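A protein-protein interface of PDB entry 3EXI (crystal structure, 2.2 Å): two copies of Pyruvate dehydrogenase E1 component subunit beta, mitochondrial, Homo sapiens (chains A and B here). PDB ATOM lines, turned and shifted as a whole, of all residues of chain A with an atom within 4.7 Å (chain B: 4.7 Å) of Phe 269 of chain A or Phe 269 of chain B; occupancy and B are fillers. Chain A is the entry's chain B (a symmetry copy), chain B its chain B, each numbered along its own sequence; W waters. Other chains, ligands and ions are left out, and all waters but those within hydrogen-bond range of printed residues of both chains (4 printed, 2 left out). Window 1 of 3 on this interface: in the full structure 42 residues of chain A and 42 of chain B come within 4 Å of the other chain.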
ATOM      1  N   ALA A 134       0.283 -19.064 -16.311  1.00  0.00           N
ATOM      2  CA  ALA A 134       1.471 -18.230 -16.256  1.00  0.00           C
ATOM      3  C   ALA A 134       1.374 -17.052 -17.230  1.00  0.00           C
ATOM      4  O   ALA A 134       1.747 -15.946 -16.893  1.00  0.00           O
ATOM      5  CB  ALA A 134       2.775 -19.070 -16.488  1.00  0.00           C
ATOM      6  N   GLY A 137      -0.949 -14.530 -15.904  1.00  0.00           N
ATOM      7  CA  GLY A 137      -0.571 -14.115 -14.551  1.00  0.00           C
ATOM      8  C   GLY A 137       0.584 -13.141 -14.594  1.00  0.00           C
ATOM      9  O   GLY A 137       0.828 -12.418 -13.643  1.00  0.00           O
ATOM     10  N   HIS A 138       1.332 -13.158 -15.689  1.00  0.00           N
ATOM     11  CA  HIS A 138       2.489 -12.296 -15.875  1.00  0.00           C
ATOM     12  C   HIS A 138       2.131 -10.828 -16.022  1.00  0.00           C
ATOM     13  O   HIS A 138       2.996  -9.941 -15.945  1.00  0.00           O
ATOM     14  CB  HIS A 138       3.096 -12.785 -17.177  1.00  0.00           C
ATOM     15  CG  HIS A 138       4.351 -12.120 -17.622  1.00  0.00           C
ATOM     16  ND1 HIS A 138       5.535 -12.226 -16.929  1.00  0.00           N
ATOM     17  CD2 HIS A 138       4.664 -11.518 -18.797  1.00  0.00           C
ATOM     18  CE1 HIS A 138       6.521 -11.670 -17.628  1.00  0.00           C
ATOM     19  NE2 HIS A 138       6.014 -11.224 -18.767  1.00  0.00           N
ATOM     20  N   ILE A 241      -4.241 -16.696  -9.290  1.00  0.00           N
ATOM     21  CA  ILE A 241      -2.892 -16.745  -9.879  1.00  0.00           C
ATOM     22  C   ILE A 241      -2.215 -15.357  -9.781  1.00  0.00           C
ATOM     23  O   ILE A 241      -1.018 -15.257  -9.452  1.00  0.00           O
ATOM     24  CB  ILE A 241      -2.961 -17.212 -11.363  1.00  0.00           C
ATOM     25  CG1 ILE A 241      -3.646 -18.582 -11.498  1.00  0.00           C
ATOM     26  CG2 ILE A 241      -1.541 -17.187 -12.035  1.00  0.00           C
ATOM     27  CD1 ILE A 241      -3.073 -19.688 -10.601  1.00  0.00           C
ATOM     28  N   MET A 244      -1.206 -13.489  -6.481  1.00  0.00           N
ATOM     29  CA  MET A 244      -1.283 -14.756  -5.737  1.00  0.00           C
ATOM     30  C   MET A 244      -1.061 -14.494  -4.266  1.00  0.00           C
ATOM     31  O   MET A 244      -0.479 -13.490  -3.879  1.00  0.00           O
ATOM     32  CB  MET A 244      -0.257 -15.797  -6.213  1.00  0.00           C
ATOM     33  CG  MET A 244       1.206 -15.397  -5.903  1.00  0.00           C
ATOM     34  SD  MET A 244       2.360 -16.770  -6.276  1.00  0.00           S
ATOM     35  CE  MET A 244       2.452 -16.766  -8.105  1.00  0.00           C
ATOM     36  N   PRO A 267       6.069 -26.592 -17.684  1.00  0.00           N
ATOM     37  CA  PRO A 267       6.964 -26.218 -16.547  1.00  0.00           C
ATOM     38  C   PRO A 267       7.747 -24.891 -16.644  1.00  0.00           C
ATOM     39  O   PRO A 267       7.831 -24.178 -15.649  1.00  0.00           O
ATOM     40  CB  PRO A 267       7.957 -27.388 -16.494  1.00  0.00           C
ATOM     41  CG  PRO A 267       8.027 -27.886 -17.974  1.00  0.00           C
ATOM     42  CD  PRO A 267       6.600 -27.715 -18.494  1.00  0.00           C
ATOM     43  N   GLN A 268       8.307 -24.554 -17.804  1.00  0.00           N
ATOM     44  CA  GLN A 268       9.234 -23.413 -17.901  1.00  0.00           C
ATOM     45  C   GLN A 268       8.533 -22.040 -17.914  1.00  0.00           C
ATOM     46  O   GLN A 268       7.678 -21.768 -18.774  1.00  0.00           O
ATOM     47  CB  GLN A 268      10.148 -23.540 -19.115  1.00  0.00           C
ATOM     48  CG  GLN A 268      10.934 -24.866 -19.097  1.00  0.00           C
ATOM     49  CD  GLN A 268      12.032 -24.917 -20.211  1.00  0.00           C
ATOM     50  OE1 GLN A 268      12.908 -24.037 -20.274  1.00  0.00           O
ATOM     51  NE2 GLN A 268      11.979 -25.970 -21.082  1.00  0.00           N
ATOM     52  N   PHE A 269       8.926 -21.188 -16.951  1.00  0.00           N
ATOM     53  CA  PHE A 269       8.289 -19.927 -16.746  1.00  0.00           C
ATOM     54  C   PHE A 269       6.834 -20.126 -16.388  1.00  0.00           C
ATOM     55  O   PHE A 269       5.994 -19.266 -16.722  1.00  0.00           O
ATOM     56  CB  PHE A 269       8.420 -19.073 -17.986  1.00  0.00           C
ATOM     57  CG  PHE A 269       9.788 -19.179 -18.655  1.00  0.00           C
ATOM     58  CD1 PHE A 269      10.847 -18.358 -18.250  1.00  0.00           C
ATOM     59  CD2 PHE A 269      10.006 -20.077 -19.716  1.00  0.00           C
ATOM     60  CE1 PHE A 269      12.149 -18.437 -18.902  1.00  0.00           C
ATOM     61  CE2 PHE A 269      11.310 -20.154 -20.392  1.00  0.00           C
ATOM     62  CZ  PHE A 269      12.353 -19.347 -19.973  1.00  0.00           C
ATOM     63  N   GLY A 270       6.536 -21.234 -15.713  1.00  0.00           N
ATOM     64  CA  GLY A 270       5.159 -21.548 -15.312  1.00  0.00           C
ATOM     65  C   GLY A 270       4.837 -21.083 -13.926  1.00  0.00           C
ATOM     66  O   GLY A 270       5.590 -20.280 -13.355  1.00  0.00           O
ATOM     67  N   VAL A 271       3.686 -21.512 -13.391  1.00  0.00           N
ATOM     68  CA  VAL A 271       3.259 -20.986 -12.137  1.00  0.00           C
ATOM     69  C   VAL A 271       4.225 -21.371 -11.012  1.00  0.00           C
ATOM     70  O   VAL A 271       4.583 -20.533 -10.187  1.00  0.00           O
ATOM     71  CB  VAL A 271       1.789 -21.464 -11.784  1.00  0.00           C
ATOM     72  CG1 VAL A 271       1.407 -21.040 -10.397  1.00  0.00           C
ATOM     73  CG2 VAL A 271       0.856 -20.889 -12.800  1.00  0.00           C
ATOM     74  N   ALA A 273       7.338 -21.894 -11.141  1.00  0.00           N
ATOM     75  CA  ALA A 273       8.610 -21.178 -11.263  1.00  0.00           C
ATOM     76  C   ALA A 273       8.523 -19.872 -10.443  1.00  0.00           C
ATOM     77  O   ALA A 273       9.503 -19.489  -9.813  1.00  0.00           O
ATOM     78  CB  ALA A 273       8.939 -20.857 -12.720  1.00  0.00           C
ATOM     79  N   GLU A 274       7.367 -19.203 -10.471  1.00  0.00           N
ATOM     80  CA  GLU A 274       7.178 -17.961  -9.698  1.00  0.00           C
ATOM     81  C   GLU A 274       7.116 -18.241  -8.206  1.00  0.00           C
ATOM     82  O   GLU A 274       7.745 -17.498  -7.415  1.00  0.00           O
ATOM     83  CB  GLU A 274       5.874 -17.205 -10.098  1.00  0.00           C
ATOM     84  CG  GLU A 274       5.659 -15.836  -9.401  1.00  0.00           C
ATOM     85  CD  GLU A 274       6.856 -14.888  -9.575  1.00  0.00           C
ATOM     86  OE1 GLU A 274       7.612 -15.023 -10.567  1.00  0.00           O
ATOM     87  OE2 GLU A 274       7.079 -14.020  -8.698  1.00  0.00           O
ATOM     88  N   ALA B 134       9.601 -14.417 -21.448  1.00  0.00           N
ATOM     89  CA  ALA B 134       8.972 -15.504 -20.717  1.00  0.00           C
ATOM     90  C   ALA B 134       7.814 -16.116 -21.509  1.00  0.00           C
ATOM     91  O   ALA B 134       7.660 -17.320 -21.538  1.00  0.00           O
ATOM     92  CB  ALA B 134       8.521 -15.048 -19.286  1.00  0.00           C
ATOM     93  N   GLY B 137       9.134 -18.186 -24.245  1.00  0.00           N
ATOM     94  CA  GLY B 137      10.072 -19.195 -23.747  1.00  0.00           C
ATOM     95  C   GLY B 137       9.330 -20.354 -23.123  1.00  0.00           C
ATOM     96  O   GLY B 137       9.875 -21.433 -22.964  1.00  0.00           O
ATOM     97  N   HIS B 138       8.089 -20.115 -22.722  1.00  0.00           N
ATOM     98  CA  HIS B 138       7.251 -21.121 -22.088  1.00  0.00           C
ATOM     99  C   HIS B 138       6.838 -22.242 -23.025  1.00  0.00           C
ATOM    100  O   HIS B 138       6.333 -23.291 -22.595  1.00  0.00           O
ATOM    101  CB  HIS B 138       6.012 -20.347 -21.673  1.00  0.00           C
ATOM    102  CG  HIS B 138       4.965 -21.106 -20.937  1.00  0.00           C
ATOM    103  ND1 HIS B 138       5.167 -21.625 -19.679  1.00  0.00           N
ATOM    104  CD2 HIS B 138       3.639 -21.252 -21.186  1.00  0.00           C
ATOM    105  CE1 HIS B 138       4.026 -22.111 -19.199  1.00  0.00           C
ATOM    106  NE2 HIS B 138       3.080 -21.902 -20.102  1.00  0.00           N
ATOM    107  N   ILE B 241      16.818 -17.999 -24.683  1.00  0.00           N
ATOM    108  CA  ILE B 241      15.811 -18.104 -23.613  1.00  0.00           C
ATOM    109  C   ILE B 241      15.252 -19.546 -23.544  1.00  0.00           C
ATOM    110  O   ILE B 241      15.071 -20.103 -22.444  1.00  0.00           O
ATOM    111  CB  ILE B 241      14.656 -17.085 -23.849  1.00  0.00           C
ATOM    112  CG1 ILE B 241      15.179 -15.643 -23.943  1.00  0.00           C
ATOM    113  CG2 ILE B 241      13.528 -17.242 -22.768  1.00  0.00           C
ATOM    114  CD1 ILE B 241      16.073 -15.198 -22.777  1.00  0.00           C
ATOM    115  N   MET B 244      17.267 -22.776 -22.592  1.00  0.00           N
ATOM    116  CA  MET B 244      18.313 -21.946 -21.974  1.00  0.00           C
ATOM    117  C   MET B 244      19.457 -22.822 -21.524  1.00  0.00           C
ATOM    118  O   MET B 244      19.299 -24.018 -21.315  1.00  0.00           O
ATOM    119  CB  MET B 244      17.806 -21.138 -20.767  1.00  0.00           C
ATOM    120  CG  MET B 244      17.423 -22.025 -19.558  1.00  0.00           C
ATOM    121  SD  MET B 244      17.054 -21.005 -18.081  1.00  0.00           S
ATOM    122  CE  MET B 244      15.401 -20.306 -18.447  1.00  0.00           C
ATOM    123  N   PRO B 267       8.372  -8.943 -13.668  1.00  0.00           N
ATOM    124  CA  PRO B 267       8.939  -9.975 -12.748  1.00  0.00           C
ATOM    125  C   PRO B 267       8.187 -11.316 -12.607  1.00  0.00           C
ATOM    126  O   PRO B 267       8.833 -12.359 -12.576  1.00  0.00           O
ATOM    127  CB  PRO B 267       8.949  -9.257 -11.391  1.00  0.00           C
ATOM    128  CG  PRO B 267       7.755  -8.253 -11.491  1.00  0.00           C
ATOM    129  CD  PRO B 267       7.777  -7.791 -12.948  1.00  0.00           C
ATOM    130  N   GLN B 268       6.857 -11.307 -12.529  1.00  0.00           N
ATOM    131  CA  GLN B 268       6.105 -12.527 -12.188  1.00  0.00           C
ATOM    132  C   GLN B 268       5.965 -13.520 -13.358  1.00  0.00           C
ATOM    133  O   GLN B 268       5.444 -13.173 -14.431  1.00  0.00           O
ATOM    134  CB  GLN B 268       4.728 -12.191 -11.625  1.00  0.00           C
ATOM    135  CG  GLN B 268       4.827 -11.264 -10.397  1.00  0.00           C
ATOM    136  CD  GLN B 268       3.449 -11.086  -9.677  1.00  0.00           C
ATOM    137  OE1 GLN B 268       2.819 -12.077  -9.269  1.00  0.00           O
ATOM    138  NE2 GLN B 268       2.997  -9.806  -9.516  1.00  0.00           N
ATOM    139  N   PHE B 269       6.428 -14.758 -13.115  1.00  0.00           N
ATOM    140  CA  PHE B 269       6.488 -15.760 -14.131  1.00  0.00           C
ATOM    141  C   PHE B 269       7.402 -15.317 -15.251  1.00  0.00           C
ATOM    142  O   PHE B 269       7.175 -15.696 -16.418  1.00  0.00           O
ATOM    143  CB  PHE B 269       5.102 -16.048 -14.657  1.00  0.00           C
ATOM    144  CG  PHE B 269       4.032 -16.076 -13.569  1.00  0.00           C
ATOM    145  CD1 PHE B 269       3.765 -17.254 -12.861  1.00  0.00           C
ATOM    146  CD2 PHE B 269       3.268 -14.932 -13.276  1.00  0.00           C
ATOM    147  CE1 PHE B 269       2.727 -17.294 -11.836  1.00  0.00           C
ATOM    148  CE2 PHE B 269       2.208 -14.965 -12.258  1.00  0.00           C
ATOM    149  CZ  PHE B 269       1.963 -16.131 -11.554  1.00  0.00           C
ATOM    150  N   GLY B 270       8.423 -14.535 -14.909  1.00  0.00           N
ATOM    151  CA  GLY B 270       9.378 -14.030 -15.904  1.00  0.00           C
ATOM    152  C   GLY B 270      10.591 -14.897 -16.036  1.00  0.00           C
ATOM    153  O   GLY B 270      10.589 -16.038 -15.551  1.00  0.00           O
ATOM    154  N   VAL B 271      11.613 -14.410 -16.753  1.00  0.00           N
ATOM    155  CA  VAL B 271      12.732 -15.248 -17.034  1.00  0.00           C
ATOM    156  C   VAL B 271      13.477 -15.633 -15.752  1.00  0.00           C
ATOM    157  O   VAL B 271      13.837 -16.794 -15.569  1.00  0.00           O
ATOM    158  CB  VAL B 271      13.725 -14.554 -18.057  1.00  0.00           C
ATOM    159  CG1 VAL B 271      14.973 -15.369 -18.226  1.00  0.00           C
ATOM    160  CG2 VAL B 271      13.010 -14.387 -19.359  1.00  0.00           C
ATOM    161  N   ALA B 273      12.356 -16.008 -12.823  1.00  0.00           N
ATOM    162  CA  ALA B 273      11.573 -16.944 -12.013  1.00  0.00           C
ATOM    163  C   ALA B 273      11.960 -18.385 -12.410  1.00  0.00           C
ATOM    164  O   ALA B 273      12.045 -19.248 -11.543  1.00  0.00           O
ATOM    165  CB  ALA B 273      10.071 -16.737 -12.205  1.00  0.00           C
ATOM    166  N   GLU B 274      12.174 -18.630 -13.706  1.00  0.00           N
ATOM    167  CA  GLU B 274      12.577 -19.968 -14.180  1.00  0.00           C
ATOM    168  C   GLU B 274      13.999 -20.301 -13.760  1.00  0.00           C
ATOM    169  O   GLU B 274      14.253 -21.442 -13.307  1.00  0.00           O
ATOM    170  CB  GLU B 274      12.493 -20.099 -15.731  1.00  0.00           C
ATOM    171  CG  GLU B 274      12.802 -21.510 -16.297  1.00  0.00           C
ATOM    172  CD  GLU B 274      11.935 -22.606 -15.659  1.00  0.00           C
ATOM    173  OE1 GLU B 274      10.815 -22.308 -15.179  1.00  0.00           O
ATOM    174  OE2 GLU B 274      12.381 -23.776 -15.594  1.00  0.00           O
HETATM  175  O   HOH W   1       4.456  -9.593 -13.520  1.00  0.00           O
HETATM  176  O   HOH W   2       6.914 -12.495 -21.539  1.00  0.00           O
HETATM  177  O   HOH W   3       0.655 -19.944 -19.475  1.00  0.00           O
HETATM  178  O   HOH W   4       7.836 -24.974 -20.852  1.00  0.00           O
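A ring nitrogen (ND1) of His 138 of chain B is in hydrogen-bond range of the backbone carbonyl oxygen of Gln 268 of chain A (2.7 Å). The side-chain carboxylate of Glu 274 of chain B lies within hydrogen-bond range of the backbone NH of Phe 269 of chain A (2.8 Å). O of Gln 268 of chain B is in hydrogen-bond range of ND1 of His 138 of chain A, at 2.7 Å. The backbone carbonyl oxygen of Ala 273 of chain A sits close to the backbone carbonyl oxygen of Ala 273 of chain B (3.1 Å). OE1 of Glu 274 of chain A lies within hydrogen-bond range of N of Phe 269 of chain B (2.8 Å).
Gly 137 of chain A touches Phe 269 of chain B (O to CE2, 3.2 Å). Phe 269 of chain B touches Ile 241 of chain A. OE1 of Glu 274 of chain B touches O of Pro 267 of chain A, 3.6 Å away. Ile 241 of chain B touches Phe 269 of chain A. O of Phe 269 of chain A touches O of Phe 269 of chain B, 3.8 Å away. O of Gly 270 of chain B touches CD1 of Phe 269 of chain A (3.6 Å). CD1 of Phe 269 of chain B touches O of Gly 270 of chain A, 3.6 Å away. O of Pro 267 of chain B touches OE1 of Glu 274 of chain A, 3.6 Å away. Glu 274 of chain A touches Gln 268 of chain B (OE1 to CA, 3.3 Å). Glu 274 of chain A touches Ala 273 of chain B (OE1 to CB, 3.4 Å).
Ala 134 of chain A touches none of the printed residues of chain B. Of the printed residues of chain B, His 138 of chain A touches Gln 268 and Phe 269. Of chain B, only Gly 137 (3.2 Å), His 138 (3.6 Å), Ile 241 (3.7 Å), Met 244 (3.5 Å), Phe 269 (3.8 Å), Gly 270 (3.6 Å), Val 271 (3.7 Å) and Glu 274 (2.8 Å) come within 4 Å of Phe 269 of chain A. Of the printed residues of chain B, Gly 270 of chain A touches Phe 269 (3.6 Å). Of the printed residues of chain B, Glu 274 of chain A touches Pro 267, Gln 268, Phe 269 and Ala 273. Ala 134 of chain B touches none of the printed residues of chain A. Printed residues of chain A within 4 Å of Met 244 of chain B: Phe 269 (3.5 Å). Printed residues of chain A within 4 Å of Gln 268 of chain B: His 138 and Glu 274. The nearest printed residue of chain B that does not touch Ala 273 of chain A is Gly 270 of chain B (5.8 Å).
Of the 12 printed residues of chain A, 11 touch a printed residue of chain B. Printed residues of chain A that touch a printed residue of chain B: Gly 137, His 138, Ile 241, Met 244, Pro 267, Gln 268, Phe 269, Gly 270, Val 271, Ala 273 and Glu 274. Hydrophobic or aromatic side chains of chain B within 4 Å of the printed part of chain A: His 138, Ile 241, Met 244, Phe 269 and Ala 273. Among the printed residues, 24 pairs touch across the chains. Among the printed residues, no Asp or Glu carboxylate lies within 4 Å of a Lys or Arg side-chain nitrogen of the other chain.
His 138 of chain A touches Gln 268 of chain B, and with the chains exchanged Gln 268 of chain A touches His 138 of chain B. Ile 241 of chain A touches Phe 269 of chain B, and with the chains exchanged Phe 269 of chain A touches Ile 241 of chain B. Gln 268 of chain A touches Glu 274 of chain B, and with the chains exchanged Glu 274 of chain A touches Gln 268 of chain B. Phe 269 of chain A touches Glu 274 of chain B, and with the chains exchanged Glu 274 of chain A touches Phe 269 of chain B. Positions printed for both chains: 134, 137, 138, 241, 244, 267, 268, 269, 270, 271, 273 and 274. Of the 24 pairs that touch across the chains among the printed residues, 24 have their exchanged pair printed and touching as well.
Water W1 lies within hydrogen-bond range of the backbone carbonyl oxygen (O) of His 138 of chain A (2.9 Å) and the backbone NH (N) of Gln 268 of chain B (3.1 Å). Water W4 lies within hydrogen-bond range of O of His 138 of chain B (2.9 Å) and N of Gln 268 of chain A (3.1 Å). Water W2 bridges NE2 of His 138 of chain A (3.2 Å) and N of Ala 134 of chain B (3.3 Å). Water W3 bridges NE2 of His 138 of chain B (3.2 Å) and N of Ala 134 of chain A (3.3 Å).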
